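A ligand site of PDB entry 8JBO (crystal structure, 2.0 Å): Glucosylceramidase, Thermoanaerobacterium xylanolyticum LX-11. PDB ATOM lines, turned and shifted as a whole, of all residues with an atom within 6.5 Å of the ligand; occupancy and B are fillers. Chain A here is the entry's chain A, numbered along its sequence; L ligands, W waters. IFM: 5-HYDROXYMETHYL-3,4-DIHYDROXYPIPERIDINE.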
ATOM      1  N   GLU A 425      -1.220 -19.501 -22.687  1.00  0.00           N
ATOM      2  CA  GLU A 425      -2.026 -20.464 -23.423  1.00  0.00           C
ATOM      3  C   GLU A 425      -3.523 -20.063 -23.364  1.00  0.00           C
ATOM      4  O   GLU A 425      -4.188 -19.988 -24.379  1.00  0.00           O
ATOM      5  CB  GLU A 425      -1.807 -21.853 -22.871  1.00  0.00           C
ATOM      6  CG  GLU A 425      -2.567 -22.936 -23.623  1.00  0.00           C
ATOM      7  CD  GLU A 425      -2.448 -24.311 -23.033  1.00  0.00           C
ATOM      8  OE1 GLU A 425      -1.392 -24.642 -22.435  1.00  0.00           O
ATOM      9  OE2 GLU A 425      -3.397 -25.089 -23.267  1.00  0.00           O
ATOM     10  N   TYR A 429      -6.077 -23.018 -18.491  1.00  0.00           N
ATOM     11  CA  TYR A 429      -4.819 -23.728 -18.493  1.00  0.00           C
ATOM     12  C   TYR A 429      -3.727 -22.633 -18.404  1.00  0.00           C
ATOM     13  O   TYR A 429      -3.206 -22.160 -19.435  1.00  0.00           O
ATOM     14  CB  TYR A 429      -4.700 -24.580 -19.775  1.00  0.00           C
ATOM     15  CG  TYR A 429      -5.945 -25.395 -20.154  1.00  0.00           C
ATOM     16  CD1 TYR A 429      -6.751 -26.027 -19.179  1.00  0.00           C
ATOM     17  CD2 TYR A 429      -6.308 -25.550 -21.495  1.00  0.00           C
ATOM     18  CE1 TYR A 429      -7.884 -26.775 -19.546  1.00  0.00           C
ATOM     19  CE2 TYR A 429      -7.424 -26.286 -21.868  1.00  0.00           C
ATOM     20  CZ  TYR A 429      -8.211 -26.883 -20.898  1.00  0.00           C
ATOM     21  OH  TYR A 429      -9.323 -27.615 -21.316  1.00  0.00           O
ATOM     22  N   TYR A 431      -0.717 -21.334 -18.386  1.00  0.00           N
ATOM     23  CA  TYR A 431       0.695 -21.617 -18.711  1.00  0.00           C
ATOM     24  C   TYR A 431       1.261 -20.616 -19.735  1.00  0.00           C
ATOM     25  O   TYR A 431       0.635 -20.379 -20.746  1.00  0.00           O
ATOM     26  CB  TYR A 431       0.837 -23.020 -19.302  1.00  0.00           C
ATOM     27  CG  TYR A 431       0.127 -24.069 -18.485  1.00  0.00           C
ATOM     28  CD1 TYR A 431       0.449 -24.249 -17.148  1.00  0.00           C
ATOM     29  CD2 TYR A 431      -0.865 -24.897 -19.049  1.00  0.00           C
ATOM     30  CE1 TYR A 431      -0.187 -25.195 -16.384  1.00  0.00           C
ATOM     31  CE2 TYR A 431      -1.511 -25.861 -18.283  1.00  0.00           C
ATOM     32  CZ  TYR A 431      -1.175 -25.979 -16.944  1.00  0.00           C
ATOM     33  OH  TYR A 431      -1.799 -26.927 -16.131  1.00  0.00           O
ATOM     34  N   THR A 434       3.007 -21.892 -23.826  1.00  0.00           N
ATOM     35  CA  THR A 434       2.897 -23.270 -24.219  1.00  0.00           C
ATOM     36  C   THR A 434       3.377 -23.512 -25.651  1.00  0.00           C
ATOM     37  O   THR A 434       2.736 -23.085 -26.595  1.00  0.00           O
ATOM     38  CB  THR A 434       1.468 -23.768 -24.059  1.00  0.00           C
ATOM     39  OG1 THR A 434       1.092 -23.591 -22.695  1.00  0.00           O
ATOM     40  CG2 THR A 434       1.393 -25.219 -24.423  1.00  0.00           C
ATOM     41  N   ASP A 436       3.844 -26.171 -27.830  1.00  0.00           N
ATOM     42  CA  ASP A 436       3.048 -26.933 -28.754  1.00  0.00           C
ATOM     43  C   ASP A 436       1.826 -26.146 -29.292  1.00  0.00           C
ATOM     44  O   ASP A 436       1.308 -26.494 -30.365  1.00  0.00           O
ATOM     45  CB  ASP A 436       2.596 -28.267 -28.161  1.00  0.00           C
ATOM     46  CG  ASP A 436       1.882 -28.092 -26.841  1.00  0.00           C
ATOM     47  OD1 ASP A 436       2.587 -27.691 -25.891  1.00  0.00           O
ATOM     48  OD2 ASP A 436       0.654 -28.331 -26.750  1.00  0.00           O
ATOM     49  N   VAL A 437       1.395 -25.129 -28.553  1.00  0.00           N
ATOM     50  CA  VAL A 437       0.310 -24.226 -28.927  1.00  0.00           C
ATOM     51  C   VAL A 437       0.843 -23.004 -29.695  1.00  0.00           C
ATOM     52  O   VAL A 437       0.257 -22.629 -30.716  1.00  0.00           O
ATOM     53  CB  VAL A 437      -0.467 -23.772 -27.684  1.00  0.00           C
ATOM     54  CG1 VAL A 437      -1.573 -22.785 -28.025  1.00  0.00           C
ATOM     55  CG2 VAL A 437      -1.084 -24.962 -26.940  1.00  0.00           C
ATOM     56  N   HIS A 491       7.393 -27.718 -21.989  1.00  0.00           N
ATOM     57  CA  HIS A 491       6.015 -27.490 -22.442  1.00  0.00           C
ATOM     58  C   HIS A 491       5.669 -26.001 -22.367  1.00  0.00           C
ATOM     59  O   HIS A 491       5.001 -25.472 -23.262  1.00  0.00           O
ATOM     60  CB  HIS A 491       5.061 -28.255 -21.539  1.00  0.00           C
ATOM     61  CG  HIS A 491       3.623 -28.035 -21.854  1.00  0.00           C
ATOM     62  ND1 HIS A 491       2.847 -27.090 -21.211  1.00  0.00           N
ATOM     63  CD2 HIS A 491       2.806 -28.654 -22.738  1.00  0.00           C
ATOM     64  CE1 HIS A 491       1.612 -27.152 -21.691  1.00  0.00           C
ATOM     65  NE2 HIS A 491       1.576 -28.073 -22.633  1.00  0.00           N
ATOM     66  N   TYR A 507       2.725 -27.245 -16.446  1.00  0.00           N
ATOM     67  CA  TYR A 507       1.755 -28.221 -16.897  1.00  0.00           C
ATOM     68  C   TYR A 507       2.122 -29.634 -16.427  1.00  0.00           C
ATOM     69  O   TYR A 507       3.255 -30.062 -16.577  1.00  0.00           O
ATOM     70  CB  TYR A 507       1.677 -28.176 -18.420  1.00  0.00           C
ATOM     71  CG  TYR A 507       0.959 -29.309 -19.109  1.00  0.00           C
ATOM     72  CD1 TYR A 507      -0.418 -29.261 -19.332  1.00  0.00           C
ATOM     73  CD2 TYR A 507       1.678 -30.369 -19.631  1.00  0.00           C
ATOM     74  CE1 TYR A 507      -1.060 -30.278 -20.040  1.00  0.00           C
ATOM     75  CE2 TYR A 507       1.065 -31.386 -20.308  1.00  0.00           C
ATOM     76  CZ  TYR A 507      -0.305 -31.343 -20.535  1.00  0.00           C
ATOM     77  OH  TYR A 507      -0.885 -32.403 -21.222  1.00  0.00           O
ATOM     78  N   TRP A 515       7.253 -35.908 -24.766  1.00  0.00           N
ATOM     79  CA  TRP A 515       6.457 -35.514 -25.932  1.00  0.00           C
ATOM     80  C   TRP A 515       7.269 -35.611 -27.209  1.00  0.00           C
ATOM     81  O   TRP A 515       8.490 -35.426 -27.204  1.00  0.00           O
ATOM     82  CB  TRP A 515       5.801 -34.128 -25.761  1.00  0.00           C
ATOM     83  CG  TRP A 515       4.556 -34.164 -24.912  1.00  0.00           C
ATOM     84  CD1 TRP A 515       4.199 -35.134 -24.014  1.00  0.00           C
ATOM     85  CD2 TRP A 515       3.516 -33.176 -24.851  1.00  0.00           C
ATOM     86  NE1 TRP A 515       2.998 -34.836 -23.440  1.00  0.00           N
ATOM     87  CE2 TRP A 515       2.555 -33.636 -23.926  1.00  0.00           C
ATOM     88  CE3 TRP A 515       3.271 -31.961 -25.537  1.00  0.00           C
ATOM     89  CZ2 TRP A 515       1.380 -32.928 -23.652  1.00  0.00           C
ATOM     90  CZ3 TRP A 515       2.116 -31.261 -25.240  1.00  0.00           C
ATOM     91  CH2 TRP A 515       1.187 -31.738 -24.310  1.00  0.00           C
ATOM     92  N   GLN A 574       1.797 -35.495 -27.116  1.00  0.00           N
ATOM     93  CA  GLN A 574       1.845 -34.345 -28.047  1.00  0.00           C
ATOM     94  C   GLN A 574       0.657 -33.446 -27.774  1.00  0.00           C
ATOM     95  O   GLN A 574      -0.133 -33.739 -26.871  1.00  0.00           O
ATOM     96  CB  GLN A 574       1.973 -34.811 -29.513  1.00  0.00           C
ATOM     97  CG  GLN A 574       1.214 -36.069 -29.900  1.00  0.00           C
ATOM     98  CD  GLN A 574      -0.266 -35.933 -29.675  1.00  0.00           C
ATOM     99  OE1 GLN A 574      -0.855 -34.931 -30.086  1.00  0.00           O
ATOM    100  NE2 GLN A 574      -0.880 -36.929 -29.027  1.00  0.00           N
ATOM    101  N   THR A 575       0.536 -32.353 -28.523  1.00  0.00           N
ATOM    102  CA  THR A 575      -0.445 -31.300 -28.214  1.00  0.00           C
ATOM    103  C   THR A 575      -1.886 -31.790 -28.036  1.00  0.00           C
ATOM    104  O   THR A 575      -2.638 -31.232 -27.246  1.00  0.00           O
ATOM    105  CB  THR A 575      -0.398 -30.180 -29.303  1.00  0.00           C
ATOM    106  OG1 THR A 575      -0.944 -28.974 -28.775  1.00  0.00           O
ATOM    107  CG2 THR A 575      -1.093 -30.589 -30.559  1.00  0.00           C
ATOM    108  N   TYR A 576      -2.255 -32.831 -28.741  1.00  0.00           N
ATOM    109  CA  TYR A 576      -3.575 -33.445 -28.559  1.00  0.00           C
ATOM    110  C   TYR A 576      -3.472 -34.341 -27.308  1.00  0.00           C
ATOM    111  O   TYR A 576      -3.362 -35.554 -27.414  1.00  0.00           O
ATOM    112  CB  TYR A 576      -4.018 -34.213 -29.824  1.00  0.00           C
ATOM    113  CG  TYR A 576      -4.146 -33.371 -31.060  1.00  0.00           C
ATOM    114  CD1 TYR A 576      -3.047 -33.136 -31.880  1.00  0.00           C
ATOM    115  CD2 TYR A 576      -5.335 -32.786 -31.407  1.00  0.00           C
ATOM    116  CE1 TYR A 576      -3.149 -32.354 -33.025  1.00  0.00           C
ATOM    117  CE2 TYR A 576      -5.452 -31.982 -32.531  1.00  0.00           C
ATOM    118  CZ  TYR A 576      -4.380 -31.777 -33.343  1.00  0.00           C
ATOM    119  OH  TYR A 576      -4.469 -30.979 -34.480  1.00  0.00           O
ATOM    120  N   ASP A 577      -3.489 -33.698 -26.146  1.00  0.00           N
ATOM    121  CA  ASP A 577      -3.000 -34.293 -24.910  1.00  0.00           C
ATOM    122  C   ASP A 577      -3.970 -35.293 -24.221  1.00  0.00           C
ATOM    123  O   ASP A 577      -3.690 -35.708 -23.120  1.00  0.00           O
ATOM    124  CB  ASP A 577      -2.462 -33.211 -23.945  1.00  0.00           C
ATOM    125  CG  ASP A 577      -3.534 -32.387 -23.281  1.00  0.00           C
ATOM    126  OD1 ASP A 577      -4.701 -32.370 -23.749  1.00  0.00           O
ATOM    127  OD2 ASP A 577      -3.203 -31.724 -22.267  1.00  0.00           O
ATOM    128  N   GLN A 711     -11.119 -35.196 -28.118  1.00  0.00           N
ATOM    129  CA  GLN A 711     -10.368 -34.288 -28.963  1.00  0.00           C
ATOM    130  C   GLN A 711     -10.546 -34.585 -30.442  1.00  0.00           C
ATOM    131  O   GLN A 711     -10.567 -33.658 -31.249  1.00  0.00           O
ATOM    132  CB  GLN A 711      -8.896 -34.265 -28.575  1.00  0.00           C
ATOM    133  CG  GLN A 711      -8.688 -33.676 -27.203  1.00  0.00           C
ATOM    134  CD  GLN A 711      -7.238 -33.593 -26.807  1.00  0.00           C
ATOM    135  OE1 GLN A 711      -6.383 -34.364 -27.263  1.00  0.00           O
ATOM    136  NE2 GLN A 711      -6.954 -32.677 -25.903  1.00  0.00           N
ATOM    137  N   GLU A 714     -13.657 -32.774 -31.564  1.00  0.00           N
ATOM    138  CA  GLU A 714     -13.629 -31.329 -31.468  1.00  0.00           C
ATOM    139  C   GLU A 714     -13.089 -30.715 -32.766  1.00  0.00           C
ATOM    140  O   GLU A 714     -12.252 -31.311 -33.479  1.00  0.00           O
ATOM    141  CB  GLU A 714     -12.748 -30.874 -30.304  1.00  0.00           C
ATOM    142  CG  GLU A 714     -13.281 -31.192 -28.901  1.00  0.00           C
ATOM    143  CD  GLU A 714     -12.310 -30.780 -27.784  1.00  0.00           C
ATOM    144  OE1 GLU A 714     -11.069 -30.891 -27.952  1.00  0.00           O
ATOM    145  OE2 GLU A 714     -12.803 -30.311 -26.726  1.00  0.00           O
ATOM    146  N   TRP A 716     -10.729 -27.683 -33.576  1.00  0.00           N
ATOM    147  CA  TRP A 716      -9.817 -26.763 -32.906  1.00  0.00           C
ATOM    148  C   TRP A 716      -9.640 -25.545 -33.821  1.00  0.00           C
ATOM    149  O   TRP A 716      -9.143 -25.669 -34.955  1.00  0.00           O
ATOM    150  CB  TRP A 716      -8.484 -27.443 -32.594  1.00  0.00           C
ATOM    151  CG  TRP A 716      -8.513 -28.369 -31.431  1.00  0.00           C
ATOM    152  CD1 TRP A 716      -9.610 -28.919 -30.843  1.00  0.00           C
ATOM    153  CD2 TRP A 716      -7.375 -28.918 -30.745  1.00  0.00           C
ATOM    154  NE1 TRP A 716      -9.244 -29.738 -29.837  1.00  0.00           N
ATOM    155  CE2 TRP A 716      -7.876 -29.773 -29.742  1.00  0.00           C
ATOM    156  CE3 TRP A 716      -5.996 -28.769 -30.885  1.00  0.00           C
ATOM    157  CZ2 TRP A 716      -7.037 -30.465 -28.848  1.00  0.00           C
ATOM    158  CZ3 TRP A 716      -5.168 -29.445 -30.005  1.00  0.00           C
ATOM    159  CH2 TRP A 716      -5.696 -30.282 -28.977  1.00  0.00           C
ATOM    160  N   GLU A 761     -10.321 -22.656 -27.648  1.00  0.00           N
ATOM    161  CA  GLU A 761      -9.552 -23.730 -28.250  1.00  0.00           C
ATOM    162  C   GLU A 761     -10.473 -24.495 -29.206  1.00  0.00           C
ATOM    163  O   GLU A 761     -10.115 -24.705 -30.355  1.00  0.00           O
ATOM    164  CB  GLU A 761      -8.983 -24.687 -27.168  1.00  0.00           C
ATOM    165  CG  GLU A 761      -8.508 -26.067 -27.654  1.00  0.00           C
ATOM    166  CD  GLU A 761      -7.075 -26.052 -28.182  1.00  0.00           C
ATOM    167  OE1 GLU A 761      -6.798 -25.459 -29.250  1.00  0.00           O
ATOM    168  OE2 GLU A 761      -6.203 -26.688 -27.528  1.00  0.00           O
ATOM    169  N   ALA A 762     -11.643 -24.924 -28.701  1.00  0.00           N
ATOM    170  CA  ALA A 762     -12.376 -26.017 -29.322  1.00  0.00           C
ATOM    171  C   ALA A 762     -13.869 -25.926 -29.141  1.00  0.00           C
ATOM    172  O   ALA A 762     -14.342 -25.351 -28.166  1.00  0.00           O
ATOM    173  CB  ALA A 762     -11.887 -27.359 -28.755  1.00  0.00           C
ATOM    174  N   ARG A 770     -14.652 -25.549 -25.308  1.00  0.00           N
ATOM    175  CA  ARG A 770     -13.653 -25.785 -24.281  1.00  0.00           C
ATOM    176  C   ARG A 770     -12.557 -24.704 -24.384  1.00  0.00           C
ATOM    177  O   ARG A 770     -12.019 -24.443 -25.475  1.00  0.00           O
ATOM    178  CB  ARG A 770     -13.046 -27.176 -24.441  1.00  0.00           C
ATOM    179  CG  ARG A 770     -11.994 -27.522 -23.410  1.00  0.00           C
ATOM    180  CD  ARG A 770     -11.635 -28.997 -23.500  1.00  0.00           C
ATOM    181  NE  ARG A 770     -10.999 -29.371 -24.734  1.00  0.00           N
ATOM    182  CZ  ARG A 770      -9.719 -29.196 -25.013  1.00  0.00           C
ATOM    183  NH1 ARG A 770      -8.884 -28.600 -24.141  1.00  0.00           N
ATOM    184  NH2 ARG A 770      -9.234 -29.592 -26.169  1.00  0.00           N
ATOM    185  N   ALA A 771     -12.308 -24.063 -23.257  1.00  0.00           N
ATOM    186  CA  ALA A 771     -11.215 -23.125 -23.035  1.00  0.00           C
ATOM    187  C   ALA A 771     -11.371 -21.850 -23.865  1.00  0.00           C
ATOM    188  O   ALA A 771     -10.676 -21.643 -24.869  1.00  0.00           O
ATOM    189  CB  ALA A 771      -9.845 -23.774 -23.258  1.00  0.00           C
ATOM    190  N   TYR A 774      -8.266 -18.257 -25.942  1.00  0.00           N
ATOM    191  CA  TYR A 774      -7.235 -19.218 -26.217  1.00  0.00           C
ATOM    192  C   TYR A 774      -6.221 -18.693 -27.214  1.00  0.00           C
ATOM    193  O   TYR A 774      -6.588 -17.990 -28.136  1.00  0.00           O
ATOM    194  CB  TYR A 774      -7.881 -20.509 -26.739  1.00  0.00           C
ATOM    195  CG  TYR A 774      -7.010 -21.695 -26.460  1.00  0.00           C
ATOM    196  CD1 TYR A 774      -6.925 -22.232 -25.174  1.00  0.00           C
ATOM    197  CD2 TYR A 774      -6.259 -22.266 -27.452  1.00  0.00           C
ATOM    198  CE1 TYR A 774      -6.080 -23.325 -24.904  1.00  0.00           C
ATOM    199  CE2 TYR A 774      -5.406 -23.318 -27.191  1.00  0.00           C
ATOM    200  CZ  TYR A 774      -5.313 -23.849 -25.920  1.00  0.00           C
ATOM    201  OH  TYR A 774      -4.432 -24.902 -25.727  1.00  0.00           O
ATOM    202  N   ARG A 776      -4.214 -20.386 -29.451  1.00  0.00           N
ATOM    203  CA  ARG A 776      -4.112 -21.059 -30.756  1.00  0.00           C
ATOM    204  C   ARG A 776      -4.745 -20.374 -32.001  1.00  0.00           C
ATOM    205  O   ARG A 776      -4.099 -20.350 -33.030  1.00  0.00           O
ATOM    206  CB  ARG A 776      -4.521 -22.537 -30.680  1.00  0.00           C
ATOM    207  CG  ARG A 776      -3.667 -23.471 -31.547  1.00  0.00           C
ATOM    208  CD  ARG A 776      -4.161 -24.916 -31.594  1.00  0.00           C
ATOM    209  NE  ARG A 776      -4.297 -25.545 -30.274  1.00  0.00           N
ATOM    210  CZ  ARG A 776      -3.385 -26.362 -29.698  1.00  0.00           C
ATOM    211  NH1 ARG A 776      -2.214 -26.671 -30.315  1.00  0.00           N
ATOM    212  NH2 ARG A 776      -3.639 -26.870 -28.495  1.00  0.00           N
HETATM  213  O4  IFM L   1      -2.430 -28.695 -26.517  1.00  0.00           O
HETATM  214  C4  IFM L   1      -2.730 -28.786 -25.114  1.00  0.00           C
HETATM  215  C3  IFM L   1      -1.659 -28.050 -24.276  1.00  0.00           C
HETATM  216  O3  IFM L   1      -0.357 -28.636 -24.481  1.00  0.00           O
HETATM  217  C2  IFM L   1      -2.018 -28.075 -22.793  1.00  0.00           C
HETATM  218  N   IFM L   1      -3.394 -27.639 -22.552  1.00  0.00           N
HETATM  219  C1  IFM L   1      -4.464 -28.277 -23.332  1.00  0.00           C
HETATM  220  C5  IFM L   1      -4.157 -28.282 -24.829  1.00  0.00           C
HETATM  221  C6  IFM L   1      -5.235 -29.117 -25.566  1.00  0.00           C
HETATM  222  O6  IFM L   1      -6.525 -28.484 -25.582  1.00  0.00           O
HETATM  223  O   HOH W   1      -4.091 -28.436 -19.863  1.00  0.00           O
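OD2 of Asp 436 lies within hydrogen-bond range of O3 of the ligand, at 2.5 Å. The backbone carbonyl oxygen (O) of Thr 575 sits at hydrogen-bond distance from an oxygen (O4) of the ligand. O4 of the ligand sits at hydrogen-bond distance from OG1 of Thr 575. N of the ligand is in salt-bridge range of OE2 of Glu 425, at 2.6 Å. The side-chain carboxylate (OE2) of Glu 761 is in hydrogen-bond range of an oxygen (O6) of the ligand, at 2.7 Å. O3 of the ligand lies within hydrogen-bond range of NE2 of His 491 (2.7 Å). An oxygen (O6) of the ligand lies within hydrogen-bond range of the guanidinium group (NH1) of Arg 770. NH2 of Arg 776 sits at hydrogen-bond distance from O4 of the ligand, 3.0 Å away.
Merely in contact with the ligand: Trp 515, Tyr 774, Trp 716, Tyr 507, Tyr 429, Asp 577, Thr 434, Gln 711 and Val 437. Hydrophobic or aromatic side chains that line the ligand: Tyr 429, Val 437, His 491, Tyr 507, Trp 515 and Trp 716. Within 4 Å of the ligand: Glu 425, Tyr 429, Thr 434, Asp 436, Val 437, His 491, Tyr 507, Trp 515, Thr 575, Asp 577, Gln 711, Trp 716, Glu 761, Arg 770, Tyr 774 and Arg 776.
The side-chain carboxylate (OD1) of Asp 436 lies close to a ring nitrogen (NE2) of His 491 (3.4 Å). The side-chain hydroxyl of Thr 575 sits at hydrogen-bond distance from the guanidinium group of Arg 776, at 3.0 Å. The backbone NH (N) of Glu 425 sits at hydrogen-bond distance from the backbone carbonyl oxygen (O) of Tyr 431 (2.8 Å). The side-chain hydroxyl (OH) of Tyr 774 sits at hydrogen-bond distance from the side-chain carboxylate (OE2) of Glu 761, at 3.1 Å. The backbone NH of Glu 761 lies within hydrogen-bond range of the backbone carbonyl oxygen of Ala 771. The backbone carbonyl oxygen of Ala 762 sits at hydrogen-bond distance from the backbone NH of Arg 770, at 2.9 Å. OE1 of Glu 714 lies within hydrogen-bond range of NE1 of Trp 716 (2.9 Å). OD1 of Asp 577 is in hydrogen-bond range of NE2 of Gln 711 (3.1 Å).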
